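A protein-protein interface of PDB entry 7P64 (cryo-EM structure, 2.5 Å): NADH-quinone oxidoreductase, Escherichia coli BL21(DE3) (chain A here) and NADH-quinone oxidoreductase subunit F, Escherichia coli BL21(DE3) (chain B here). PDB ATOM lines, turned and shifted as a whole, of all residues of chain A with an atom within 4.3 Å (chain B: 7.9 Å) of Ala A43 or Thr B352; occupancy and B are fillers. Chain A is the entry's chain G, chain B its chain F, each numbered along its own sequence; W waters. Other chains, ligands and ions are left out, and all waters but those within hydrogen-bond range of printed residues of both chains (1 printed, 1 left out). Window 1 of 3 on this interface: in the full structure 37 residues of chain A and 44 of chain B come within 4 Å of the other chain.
The backbone carbonyl oxygen (O) of Trp B350 is in hydrogen-bond range of the guanidinium group (NH1) of Arg B355 (3.5 Å). The side-chain sulfur (SG) of Cys B351 sits close to the backbone NH (N) of Phe B394 (3.3 Å). The side-chain hydroxyl of Thr B352 sits at hydrogen-bond distance from the guanidinium group of Arg B355 (3.1 Å). The guanidinium group of Arg B355 is in salt-bridge range of the side-chain carboxylate of Asp B356 (3.4 Å). The side-chain sulfur of Cys A33 lies close to the backbone NH of Ala A43 (3.2 Å). The guanidinium group (NH1) of Arg A45 lies within hydrogen-bond range of the backbone carbonyl oxygen (O) of Gly A42, at 3.1 Å.
Hydrophobic or aromatic side chains of chain A within 4 Å of the printed part of chain B: Val A41, Ala A43, Trp A93 and Leu A94. Printed residues of chain B that touch a printed residue of chain A: Trp B350, Cys B351, Thr B352, Pro B353, Arg B355, Asp B356, Gly B357, Leu B384, Phe B387, Leu B388, Lys B392, Thr B393 and Phe B394. Hydrophobic or aromatic side chains of chain B within 4 Å of the printed part of chain A: Trp B350, Pro B353, Leu B384, Phe B387, Leu B388 and Phe B394. Among the printed residues, no Asp or Glu carboxylate lies within 4 Å of a Lys or Arg side-chain nitrogen of the other chain.
Trp B350 touches Val A41. Trp B350 touches Gly A42. O of Gly A42 touches CD1 of Phe B394 (3.2 Å). CB of Ala A43 touches O of Trp B350, at 3.6 Å. Cys B351 touches Ala A43 (CA to O, 3.2 Å). Ala A43 touches Thr B352 (O to N, 3.6 Å). Arg A45 touches Pro B353. Phe B394 touches Arg A45. Trp A93 touches Asp B356 (O to CB, 3.6 Å). Trp A93 touches Leu B384 (NE1 to CD2, 3.4 Å).
OG1 of Thr B352 is in hydrogen-bond range of O of Cys A44, 2.9 Å away. The backbone carbonyl oxygen (O) of Lys B392 lies within hydrogen-bond range of the guanidinium group (NE) of Arg A45 (2.9 Å). The guanidinium group of Arg A45 sits at hydrogen-bond distance from the backbone carbonyl oxygen of Thr B393.
Water W1 lies within hydrogen-bond range of the guanidinium group (NH1) of Arg B355 (2.6 Å), the backbone carbonyl oxygen (O) of Trp B350 (2.8 Å), the side-chain hydroxyl (OG1) of Thr B352 (3.4 Å) and the backbone carbonyl oxygen (O) of Ala A43 (3.4 Å).
Of chain B, only Trp B350, Cys B351 and Thr B352 come within 4 Å of Ala A43. Thr B352 touches three residues of chain A. Of the printed residues of chain B, Leu A94 touches Thr B352 (3.7 Å), Arg B355 (3.6 Å) and Asp B356 (3.7 Å). Of the printed residues of chain A, Leu B388 touches Trp A93. Printed residues of chain A within 4 Å of Cys B351: Ala A43 (3.2 Å) and Arg A45 (3.9 Å). Ser B347 touches none of the printed residues of chain A. Val A90 touches none of the printed residues of chain B. The nearest printed residue of chain A that does not touch Lys B392 is Val A90 (6.5 Å).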
ATOM      1  N   CYS A  33      -2.353  11.470 -36.550  1.00  0.00           N
ATOM      2  CA  CYS A  33      -1.018  12.053 -36.536  1.00  0.00           C
ATOM      3  C   CYS A  33      -0.095  11.491 -37.608  1.00  0.00           C
ATOM      4  O   CYS A  33       0.960  12.080 -37.858  1.00  0.00           O
ATOM      5  CB  CYS A  33      -0.379  11.870 -35.157  1.00  0.00           C
ATOM      6  SG  CYS A  33       0.162  10.202 -34.776  1.00  0.00           S
ATOM      7  N   VAL A  41       4.724   8.905 -35.725  1.00  0.00           N
ATOM      8  CA  VAL A  41       5.176   9.385 -34.421  1.00  0.00           C
ATOM      9  C   VAL A  41       4.387   8.807 -33.259  1.00  0.00           C
ATOM     10  O   VAL A  41       4.860   8.874 -32.111  1.00  0.00           O
ATOM     11  CB  VAL A  41       5.151  10.926 -34.363  1.00  0.00           C
ATOM     12  CG1 VAL A  41       6.344  11.496 -35.094  1.00  0.00           C
ATOM     13  CG2 VAL A  41       3.846  11.463 -34.923  1.00  0.00           C
ATOM     14  N   GLY A  42       3.207   8.239 -33.479  1.00  0.00           N
ATOM     15  CA  GLY A  42       2.434   7.654 -32.399  1.00  0.00           C
ATOM     16  C   GLY A  42       1.868   8.637 -31.397  1.00  0.00           C
ATOM     17  O   GLY A  42       1.836   8.340 -30.198  1.00  0.00           O
ATOM     18  N   ALA A  43       1.398   9.792 -31.860  1.00  0.00           N
ATOM     19  CA  ALA A  43       0.905  10.828 -30.959  1.00  0.00           C
ATOM     20  C   ALA A  43      -0.591  10.693 -30.681  1.00  0.00           C
ATOM     21  O   ALA A  43      -0.996  10.560 -29.527  1.00  0.00           O
ATOM     22  CB  ALA A  43       1.224  12.211 -31.532  1.00  0.00           C
ATOM     23  N   CYS A  44      -1.420  10.712 -31.725  1.00  0.00           N
ATOM     24  CA  CYS A  44      -2.866  10.831 -31.541  1.00  0.00           C
ATOM     25  C   CYS A  44      -3.504   9.597 -30.912  1.00  0.00           C
ATOM     26  O   CYS A  44      -4.608   9.705 -30.373  1.00  0.00           O
ATOM     27  CB  CYS A  44      -3.540  11.120 -32.878  1.00  0.00           C
ATOM     28  SG  CYS A  44      -3.500   9.744 -34.025  1.00  0.00           S
ATOM     29  N   ARG A  45      -2.842   8.439 -30.984  1.00  0.00           N
ATOM     30  CA  ARG A  45      -3.315   7.165 -30.425  1.00  0.00           C
ATOM     31  C   ARG A  45      -4.649   6.724 -31.021  1.00  0.00           C
ATOM     32  O   ARG A  45      -5.419   6.009 -30.380  1.00  0.00           O
ATOM     33  CB  ARG A  45      -3.399   7.199 -28.892  1.00  0.00           C
ATOM     34  CG  ARG A  45      -2.197   7.817 -28.199  1.00  0.00           C
ATOM     35  CD  ARG A  45      -0.897   7.169 -28.595  1.00  0.00           C
ATOM     36  NE  ARG A  45      -0.698   5.882 -27.948  1.00  0.00           N
ATOM     37  CZ  ARG A  45       0.391   5.143 -28.094  1.00  0.00           C
ATOM     38  NH1 ARG A  45       1.398   5.542 -28.851  1.00  0.00           N
ATOM     39  NH2 ARG A  45       0.469   3.974 -27.467  1.00  0.00           N
ATOM     40  N   VAL A  90     -10.901   7.590 -28.103  1.00  0.00           N
ATOM     41  CA  VAL A  90      -9.947   8.610 -28.531  1.00  0.00           C
ATOM     42  C   VAL A  90     -10.663   9.733 -29.277  1.00  0.00           C
ATOM     43  O   VAL A  90     -10.395  10.923 -29.046  1.00  0.00           O
ATOM     44  CB  VAL A  90      -8.827   7.976 -29.377  1.00  0.00           C
ATOM     45  CG1 VAL A  90      -7.993   9.040 -30.057  1.00  0.00           C
ATOM     46  CG2 VAL A  90      -7.948   7.110 -28.508  1.00  0.00           C
ATOM     47  N   TRP A  93     -12.466  11.785 -26.667  1.00  0.00           N
ATOM     48  CA  TRP A  93     -11.555  12.685 -25.965  1.00  0.00           C
ATOM     49  C   TRP A  93     -11.208  13.896 -26.816  1.00  0.00           C
ATOM     50  O   TRP A  93     -11.090  15.011 -26.300  1.00  0.00           O
ATOM     51  CB  TRP A  93     -10.279  11.951 -25.570  1.00  0.00           C
ATOM     52  CG  TRP A  93     -10.460  11.003 -24.455  1.00  0.00           C
ATOM     53  CD1 TRP A  93     -11.250  11.166 -23.363  1.00  0.00           C
ATOM     54  CD2 TRP A  93      -9.838   9.728 -24.317  1.00  0.00           C
ATOM     55  NE1 TRP A  93     -11.159  10.070 -22.548  1.00  0.00           N
ATOM     56  CE2 TRP A  93     -10.297   9.170 -23.113  1.00  0.00           C
ATOM     57  CE3 TRP A  93      -8.935   9.002 -25.096  1.00  0.00           C
ATOM     58  CZ2 TRP A  93      -9.886   7.922 -22.669  1.00  0.00           C
ATOM     59  CZ3 TRP A  93      -8.532   7.763 -24.656  1.00  0.00           C
ATOM     60  CH2 TRP A  93      -9.002   7.237 -23.453  1.00  0.00           C
ATOM     61  N   LEU A  94     -11.026  13.692 -28.123  1.00  0.00           N
ATOM     62  CA  LEU A  94     -10.789  14.829 -29.007  1.00  0.00           C
ATOM     63  C   LEU A  94     -12.011  15.734 -29.111  1.00  0.00           C
ATOM     64  O   LEU A  94     -11.867  16.939 -29.334  1.00  0.00           O
ATOM     65  CB  LEU A  94     -10.371  14.342 -30.391  1.00  0.00           C
ATOM     66  CG  LEU A  94      -9.002  13.671 -30.456  1.00  0.00           C
ATOM     67  CD1 LEU A  94      -8.732  13.175 -31.854  1.00  0.00           C
ATOM     68  CD2 LEU A  94      -7.921  14.631 -30.006  1.00  0.00           C
ATOM     69  N   SER B 347       1.118  16.724 -17.571  1.00  0.00           N
ATOM     70  CA  SER B 347       1.149  16.057 -18.861  1.00  0.00           C
ATOM     71  C   SER B 347       2.029  16.837 -19.827  1.00  0.00           C
ATOM     72  O   SER B 347       2.062  18.069 -19.802  1.00  0.00           O
ATOM     73  CB  SER B 347      -0.267  15.935 -19.418  1.00  0.00           C
ATOM     74  OG  SER B 347      -0.256  15.456 -20.749  1.00  0.00           O
ATOM     75  N   GLY B 349       1.592  16.672 -23.057  1.00  0.00           N
ATOM     76  CA  GLY B 349       0.724  17.068 -24.140  1.00  0.00           C
ATOM     77  C   GLY B 349       0.908  16.320 -25.436  1.00  0.00           C
ATOM     78  O   GLY B 349       0.290  16.697 -26.437  1.00  0.00           O
ATOM     79  N   TRP B 350       1.734  15.277 -25.453  1.00  0.00           N
ATOM     80  CA  TRP B 350       2.027  14.588 -26.703  1.00  0.00           C
ATOM     81  C   TRP B 350       0.849  13.745 -27.170  1.00  0.00           C
ATOM     82  O   TRP B 350       0.487  13.774 -28.352  1.00  0.00           O
ATOM     83  CB  TRP B 350       3.269  13.720 -26.538  1.00  0.00           C
ATOM     84  CG  TRP B 350       3.660  12.967 -27.750  1.00  0.00           C
ATOM     85  CD1 TRP B 350       3.614  11.620 -27.922  1.00  0.00           C
ATOM     86  CD2 TRP B 350       4.174  13.512 -28.967  1.00  0.00           C
ATOM     87  NE1 TRP B 350       4.062  11.288 -29.171  1.00  0.00           N
ATOM     88  CE2 TRP B 350       4.414  12.432 -29.834  1.00  0.00           C
ATOM     89  CE3 TRP B 350       4.453  14.807 -29.408  1.00  0.00           C
ATOM     90  CZ2 TRP B 350       4.919  12.607 -31.117  1.00  0.00           C
ATOM     91  CZ3 TRP B 350       4.950  14.979 -30.681  1.00  0.00           C
ATOM     92  CH2 TRP B 350       5.179  13.886 -31.521  1.00  0.00           C
ATOM     93  N   CYS B 351       0.233  12.990 -26.270  1.00  0.00           N
ATOM     94  CA  CYS B 351      -0.692  11.956 -26.697  1.00  0.00           C
ATOM     95  C   CYS B 351      -2.078  12.144 -26.094  1.00  0.00           C
ATOM     96  O   CYS B 351      -2.233  12.634 -24.974  1.00  0.00           O
ATOM     97  CB  CYS B 351      -0.124  10.558 -26.397  1.00  0.00           C
ATOM     98  SG  CYS B 351      -0.233   9.937 -24.742  1.00  0.00           S
ATOM     99  N   THR B 352      -3.079  11.751 -26.886  1.00  0.00           N
ATOM    100  CA  THR B 352      -4.477  12.092 -26.617  1.00  0.00           C
ATOM    101  C   THR B 352      -5.041  11.559 -25.300  1.00  0.00           C
ATOM    102  O   THR B 352      -5.706  12.342 -24.602  1.00  0.00           O
ATOM    103  CB  THR B 352      -5.344  11.646 -27.802  1.00  0.00           C
ATOM    104  OG1 THR B 352      -4.855  12.242 -29.007  1.00  0.00           O
ATOM    105  CG2 THR B 352      -6.796  12.046 -27.602  1.00  0.00           C
ATOM    106  N   PRO B 353      -4.869  10.278 -24.909  1.00  0.00           N
ATOM    107  CA  PRO B 353      -5.553   9.814 -23.684  1.00  0.00           C
ATOM    108  C   PRO B 353      -5.147  10.557 -22.427  1.00  0.00           C
ATOM    109  O   PRO B 353      -6.022  11.021 -21.700  1.00  0.00           O
ATOM    110  CB  PRO B 353      -5.179   8.329 -23.621  1.00  0.00           C
ATOM    111  CG  PRO B 353      -4.898   7.966 -25.003  1.00  0.00           C
ATOM    112  CD  PRO B 353      -4.174   9.140 -25.538  1.00  0.00           C
ATOM    113  N   CYS B 354      -3.852  10.756 -22.197  1.00  0.00           N
ATOM    114  CA  CYS B 354      -3.411  11.530 -21.041  1.00  0.00           C
ATOM    115  C   CYS B 354      -3.877  12.979 -21.138  1.00  0.00           C
ATOM    116  O   CYS B 354      -4.639  13.446 -20.280  1.00  0.00           O
ATOM    117  CB  CYS B 354      -1.891  11.419 -20.937  1.00  0.00           C
ATOM    118  SG  CYS B 354      -0.927  12.475 -19.839  1.00  0.00           S
ATOM    119  N   ARG B 355      -3.568  13.636 -22.263  1.00  0.00           N
ATOM    120  CA  ARG B 355      -3.776  15.075 -22.426  1.00  0.00           C
ATOM    121  C   ARG B 355      -5.252  15.462 -22.366  1.00  0.00           C
ATOM    122  O   ARG B 355      -5.601  16.510 -21.813  1.00  0.00           O
ATOM    123  CB  ARG B 355      -3.158  15.533 -23.750  1.00  0.00           C
ATOM    124  CG  ARG B 355      -3.729  16.821 -24.324  1.00  0.00           C
ATOM    125  CD  ARG B 355      -3.194  17.138 -25.699  1.00  0.00           C
ATOM    126  NE  ARG B 355      -4.106  16.666 -26.730  1.00  0.00           N
ATOM    127  CZ  ARG B 355      -3.821  15.707 -27.597  1.00  0.00           C
ATOM    128  NH1 ARG B 355      -2.635  15.126 -27.618  1.00  0.00           N
ATOM    129  NH2 ARG B 355      -4.750  15.322 -28.464  1.00  0.00           N
ATOM    130  N   ASP B 356      -6.132  14.632 -22.919  1.00  0.00           N
ATOM    131  CA  ASP B 356      -7.547  14.957 -22.996  1.00  0.00           C
ATOM    132  C   ASP B 356      -8.424  14.127 -22.068  1.00  0.00           C
ATOM    133  O   ASP B 356      -9.621  14.408 -21.972  1.00  0.00           O
ATOM    134  CB  ASP B 356      -8.047  14.799 -24.434  1.00  0.00           C
ATOM    135  CG  ASP B 356      -7.628  15.946 -25.327  1.00  0.00           C
ATOM    136  OD1 ASP B 356      -7.446  17.069 -24.816  1.00  0.00           O
ATOM    137  OD2 ASP B 356      -7.485  15.726 -26.545  1.00  0.00           O
ATOM    138  N   GLY B 357      -7.875  13.142 -21.361  1.00  0.00           N
ATOM    139  CA  GLY B 357      -8.694  12.324 -20.502  1.00  0.00           C
ATOM    140  C   GLY B 357      -8.396  12.561 -19.044  1.00  0.00           C
ATOM    141  O   GLY B 357      -9.294  12.414 -18.212  1.00  0.00           O
ATOM    142  N   LEU B 358      -7.152  12.907 -18.705  1.00  0.00           N
ATOM    143  CA  LEU B 358      -6.877  13.337 -17.339  1.00  0.00           C
ATOM    144  C   LEU B 358      -7.635  14.607 -16.940  1.00  0.00           C
ATOM    145  O   LEU B 358      -8.135  14.641 -15.803  1.00  0.00           O
ATOM    146  CB  LEU B 358      -5.363  13.477 -17.134  1.00  0.00           C
ATOM    147  CG  LEU B 358      -4.591  12.158 -17.088  1.00  0.00           C
ATOM    148  CD1 LEU B 358      -3.119  12.401 -16.833  1.00  0.00           C
ATOM    149  CD2 LEU B 358      -5.170  11.234 -16.032  1.00  0.00           C
ATOM    150  N   PRO B 359      -7.755  15.662 -17.767  1.00  0.00           N
ATOM    151  CA  PRO B 359      -8.645  16.773 -17.380  1.00  0.00           C
ATOM    152  C   PRO B 359     -10.106  16.384 -17.220  1.00  0.00           C
ATOM    153  O   PRO B 359     -10.798  16.978 -16.386  1.00  0.00           O
ATOM    154  CB  PRO B 359      -8.457  17.782 -18.519  1.00  0.00           C
ATOM    155  CG  PRO B 359      -7.118  17.521 -19.010  1.00  0.00           C
ATOM    156  CD  PRO B 359      -6.964  16.044 -18.953  1.00  0.00           C
ATOM    157  N   LEU B 384     -11.751   5.447 -18.116  1.00  0.00           N
ATOM    158  CA  LEU B 384     -10.464   6.130 -18.199  1.00  0.00           C
ATOM    159  C   LEU B 384      -9.345   5.274 -17.620  1.00  0.00           C
ATOM    160  O   LEU B 384      -8.224   5.282 -18.133  1.00  0.00           O
ATOM    161  CB  LEU B 384     -10.537   7.475 -17.477  1.00  0.00           C
ATOM    162  CG  LEU B 384     -11.312   8.589 -18.185  1.00  0.00           C
ATOM    163  CD1 LEU B 384     -11.692   9.685 -17.208  1.00  0.00           C
ATOM    164  CD2 LEU B 384     -10.499   9.159 -19.327  1.00  0.00           C
ATOM    165  N   PHE B 387      -8.619   2.602 -20.334  1.00  0.00           N
ATOM    166  CA  PHE B 387      -8.086   3.084 -21.600  1.00  0.00           C
ATOM    167  C   PHE B 387      -6.877   4.001 -21.453  1.00  0.00           C
ATOM    168  O   PHE B 387      -6.375   4.500 -22.463  1.00  0.00           O
ATOM    169  CB  PHE B 387      -9.187   3.793 -22.388  1.00  0.00           C
ATOM    170  CG  PHE B 387     -10.158   2.852 -23.037  1.00  0.00           C
ATOM    171  CD1 PHE B 387      -9.766   1.572 -23.391  1.00  0.00           C
ATOM    172  CD2 PHE B 387     -11.460   3.239 -23.283  1.00  0.00           C
ATOM    173  CE1 PHE B 387     -10.652   0.701 -23.985  1.00  0.00           C
ATOM    174  CE2 PHE B 387     -12.352   2.369 -23.876  1.00  0.00           C
ATOM    175  CZ  PHE B 387     -11.946   1.102 -24.228  1.00  0.00           C
ATOM    176  N   LEU B 388      -6.394   4.237 -20.234  1.00  0.00           N
ATOM    177  CA  LEU B 388      -5.132   4.935 -20.027  1.00  0.00           C
ATOM    178  C   LEU B 388      -4.057   4.010 -19.472  1.00  0.00           C
ATOM    179  O   LEU B 388      -3.061   4.483 -18.920  1.00  0.00           O
ATOM    180  CB  LEU B 388      -5.316   6.140 -19.106  1.00  0.00           C
ATOM    181  CG  LEU B 388      -5.555   7.499 -19.763  1.00  0.00           C
ATOM    182  CD1 LEU B 388      -6.992   7.628 -20.233  1.00  0.00           C
ATOM    183  CD2 LEU B 388      -5.204   8.619 -18.803  1.00  0.00           C
ATOM    184  N   LYS B 392      -1.509   2.030 -24.177  1.00  0.00           N
ATOM    185  CA  LYS B 392      -2.512   2.903 -24.771  1.00  0.00           C
ATOM    186  C   LYS B 392      -2.039   4.344 -24.881  1.00  0.00           C
ATOM    187  O   LYS B 392      -2.460   5.059 -25.795  1.00  0.00           O
ATOM    188  CB  LYS B 392      -3.808   2.846 -23.958  1.00  0.00           C
ATOM    189  CG  LYS B 392      -4.688   1.652 -24.281  1.00  0.00           C
ATOM    190  CD  LYS B 392      -4.498   0.536 -23.278  1.00  0.00           C
ATOM    191  CE  LYS B 392      -5.537  -0.551 -23.462  1.00  0.00           C
ATOM    192  NZ  LYS B 392      -5.330  -1.661 -22.496  1.00  0.00           N
ATOM    193  N   THR B 393      -1.180   4.785 -23.971  1.00  0.00           N
ATOM    194  CA  THR B 393      -0.561   6.097 -24.048  1.00  0.00           C
ATOM    195  C   THR B 393       0.878   5.965 -24.530  1.00  0.00           C
ATOM    196  O   THR B 393       1.449   4.875 -24.582  1.00  0.00           O
ATOM    197  CB  THR B 393      -0.614   6.799 -22.692  1.00  0.00           C
ATOM    198  OG1 THR B 393       0.085   6.015 -21.719  1.00  0.00           O
ATOM    199  CG2 THR B 393      -2.048   6.962 -22.257  1.00  0.00           C
ATOM    200  N   PHE B 394       1.465   7.106 -24.889  1.00  0.00           N
ATOM    201  CA  PHE B 394       2.799   7.093 -25.476  1.00  0.00           C
ATOM    202  C   PHE B 394       3.874   6.783 -24.443  1.00  0.00           C
ATOM    203  O   PHE B 394       4.918   6.221 -24.791  1.00  0.00           O
ATOM    204  CB  PHE B 394       3.078   8.428 -26.157  1.00  0.00           C
ATOM    205  CG  PHE B 394       4.307   8.427 -27.012  1.00  0.00           C
ATOM    206  CD1 PHE B 394       4.300   7.822 -28.254  1.00  0.00           C
ATOM    207  CD2 PHE B 394       5.469   9.035 -26.574  1.00  0.00           C
ATOM    208  CE1 PHE B 394       5.425   7.824 -29.045  1.00  0.00           C
ATOM    209  CE2 PHE B 394       6.597   9.039 -27.360  1.00  0.00           C
ATOM    210  CZ  PHE B 394       6.576   8.434 -28.597  1.00  0.00           C
HETATM  211  O   HOH W   1      -1.940  13.862 -29.736  1.00  0.00           O
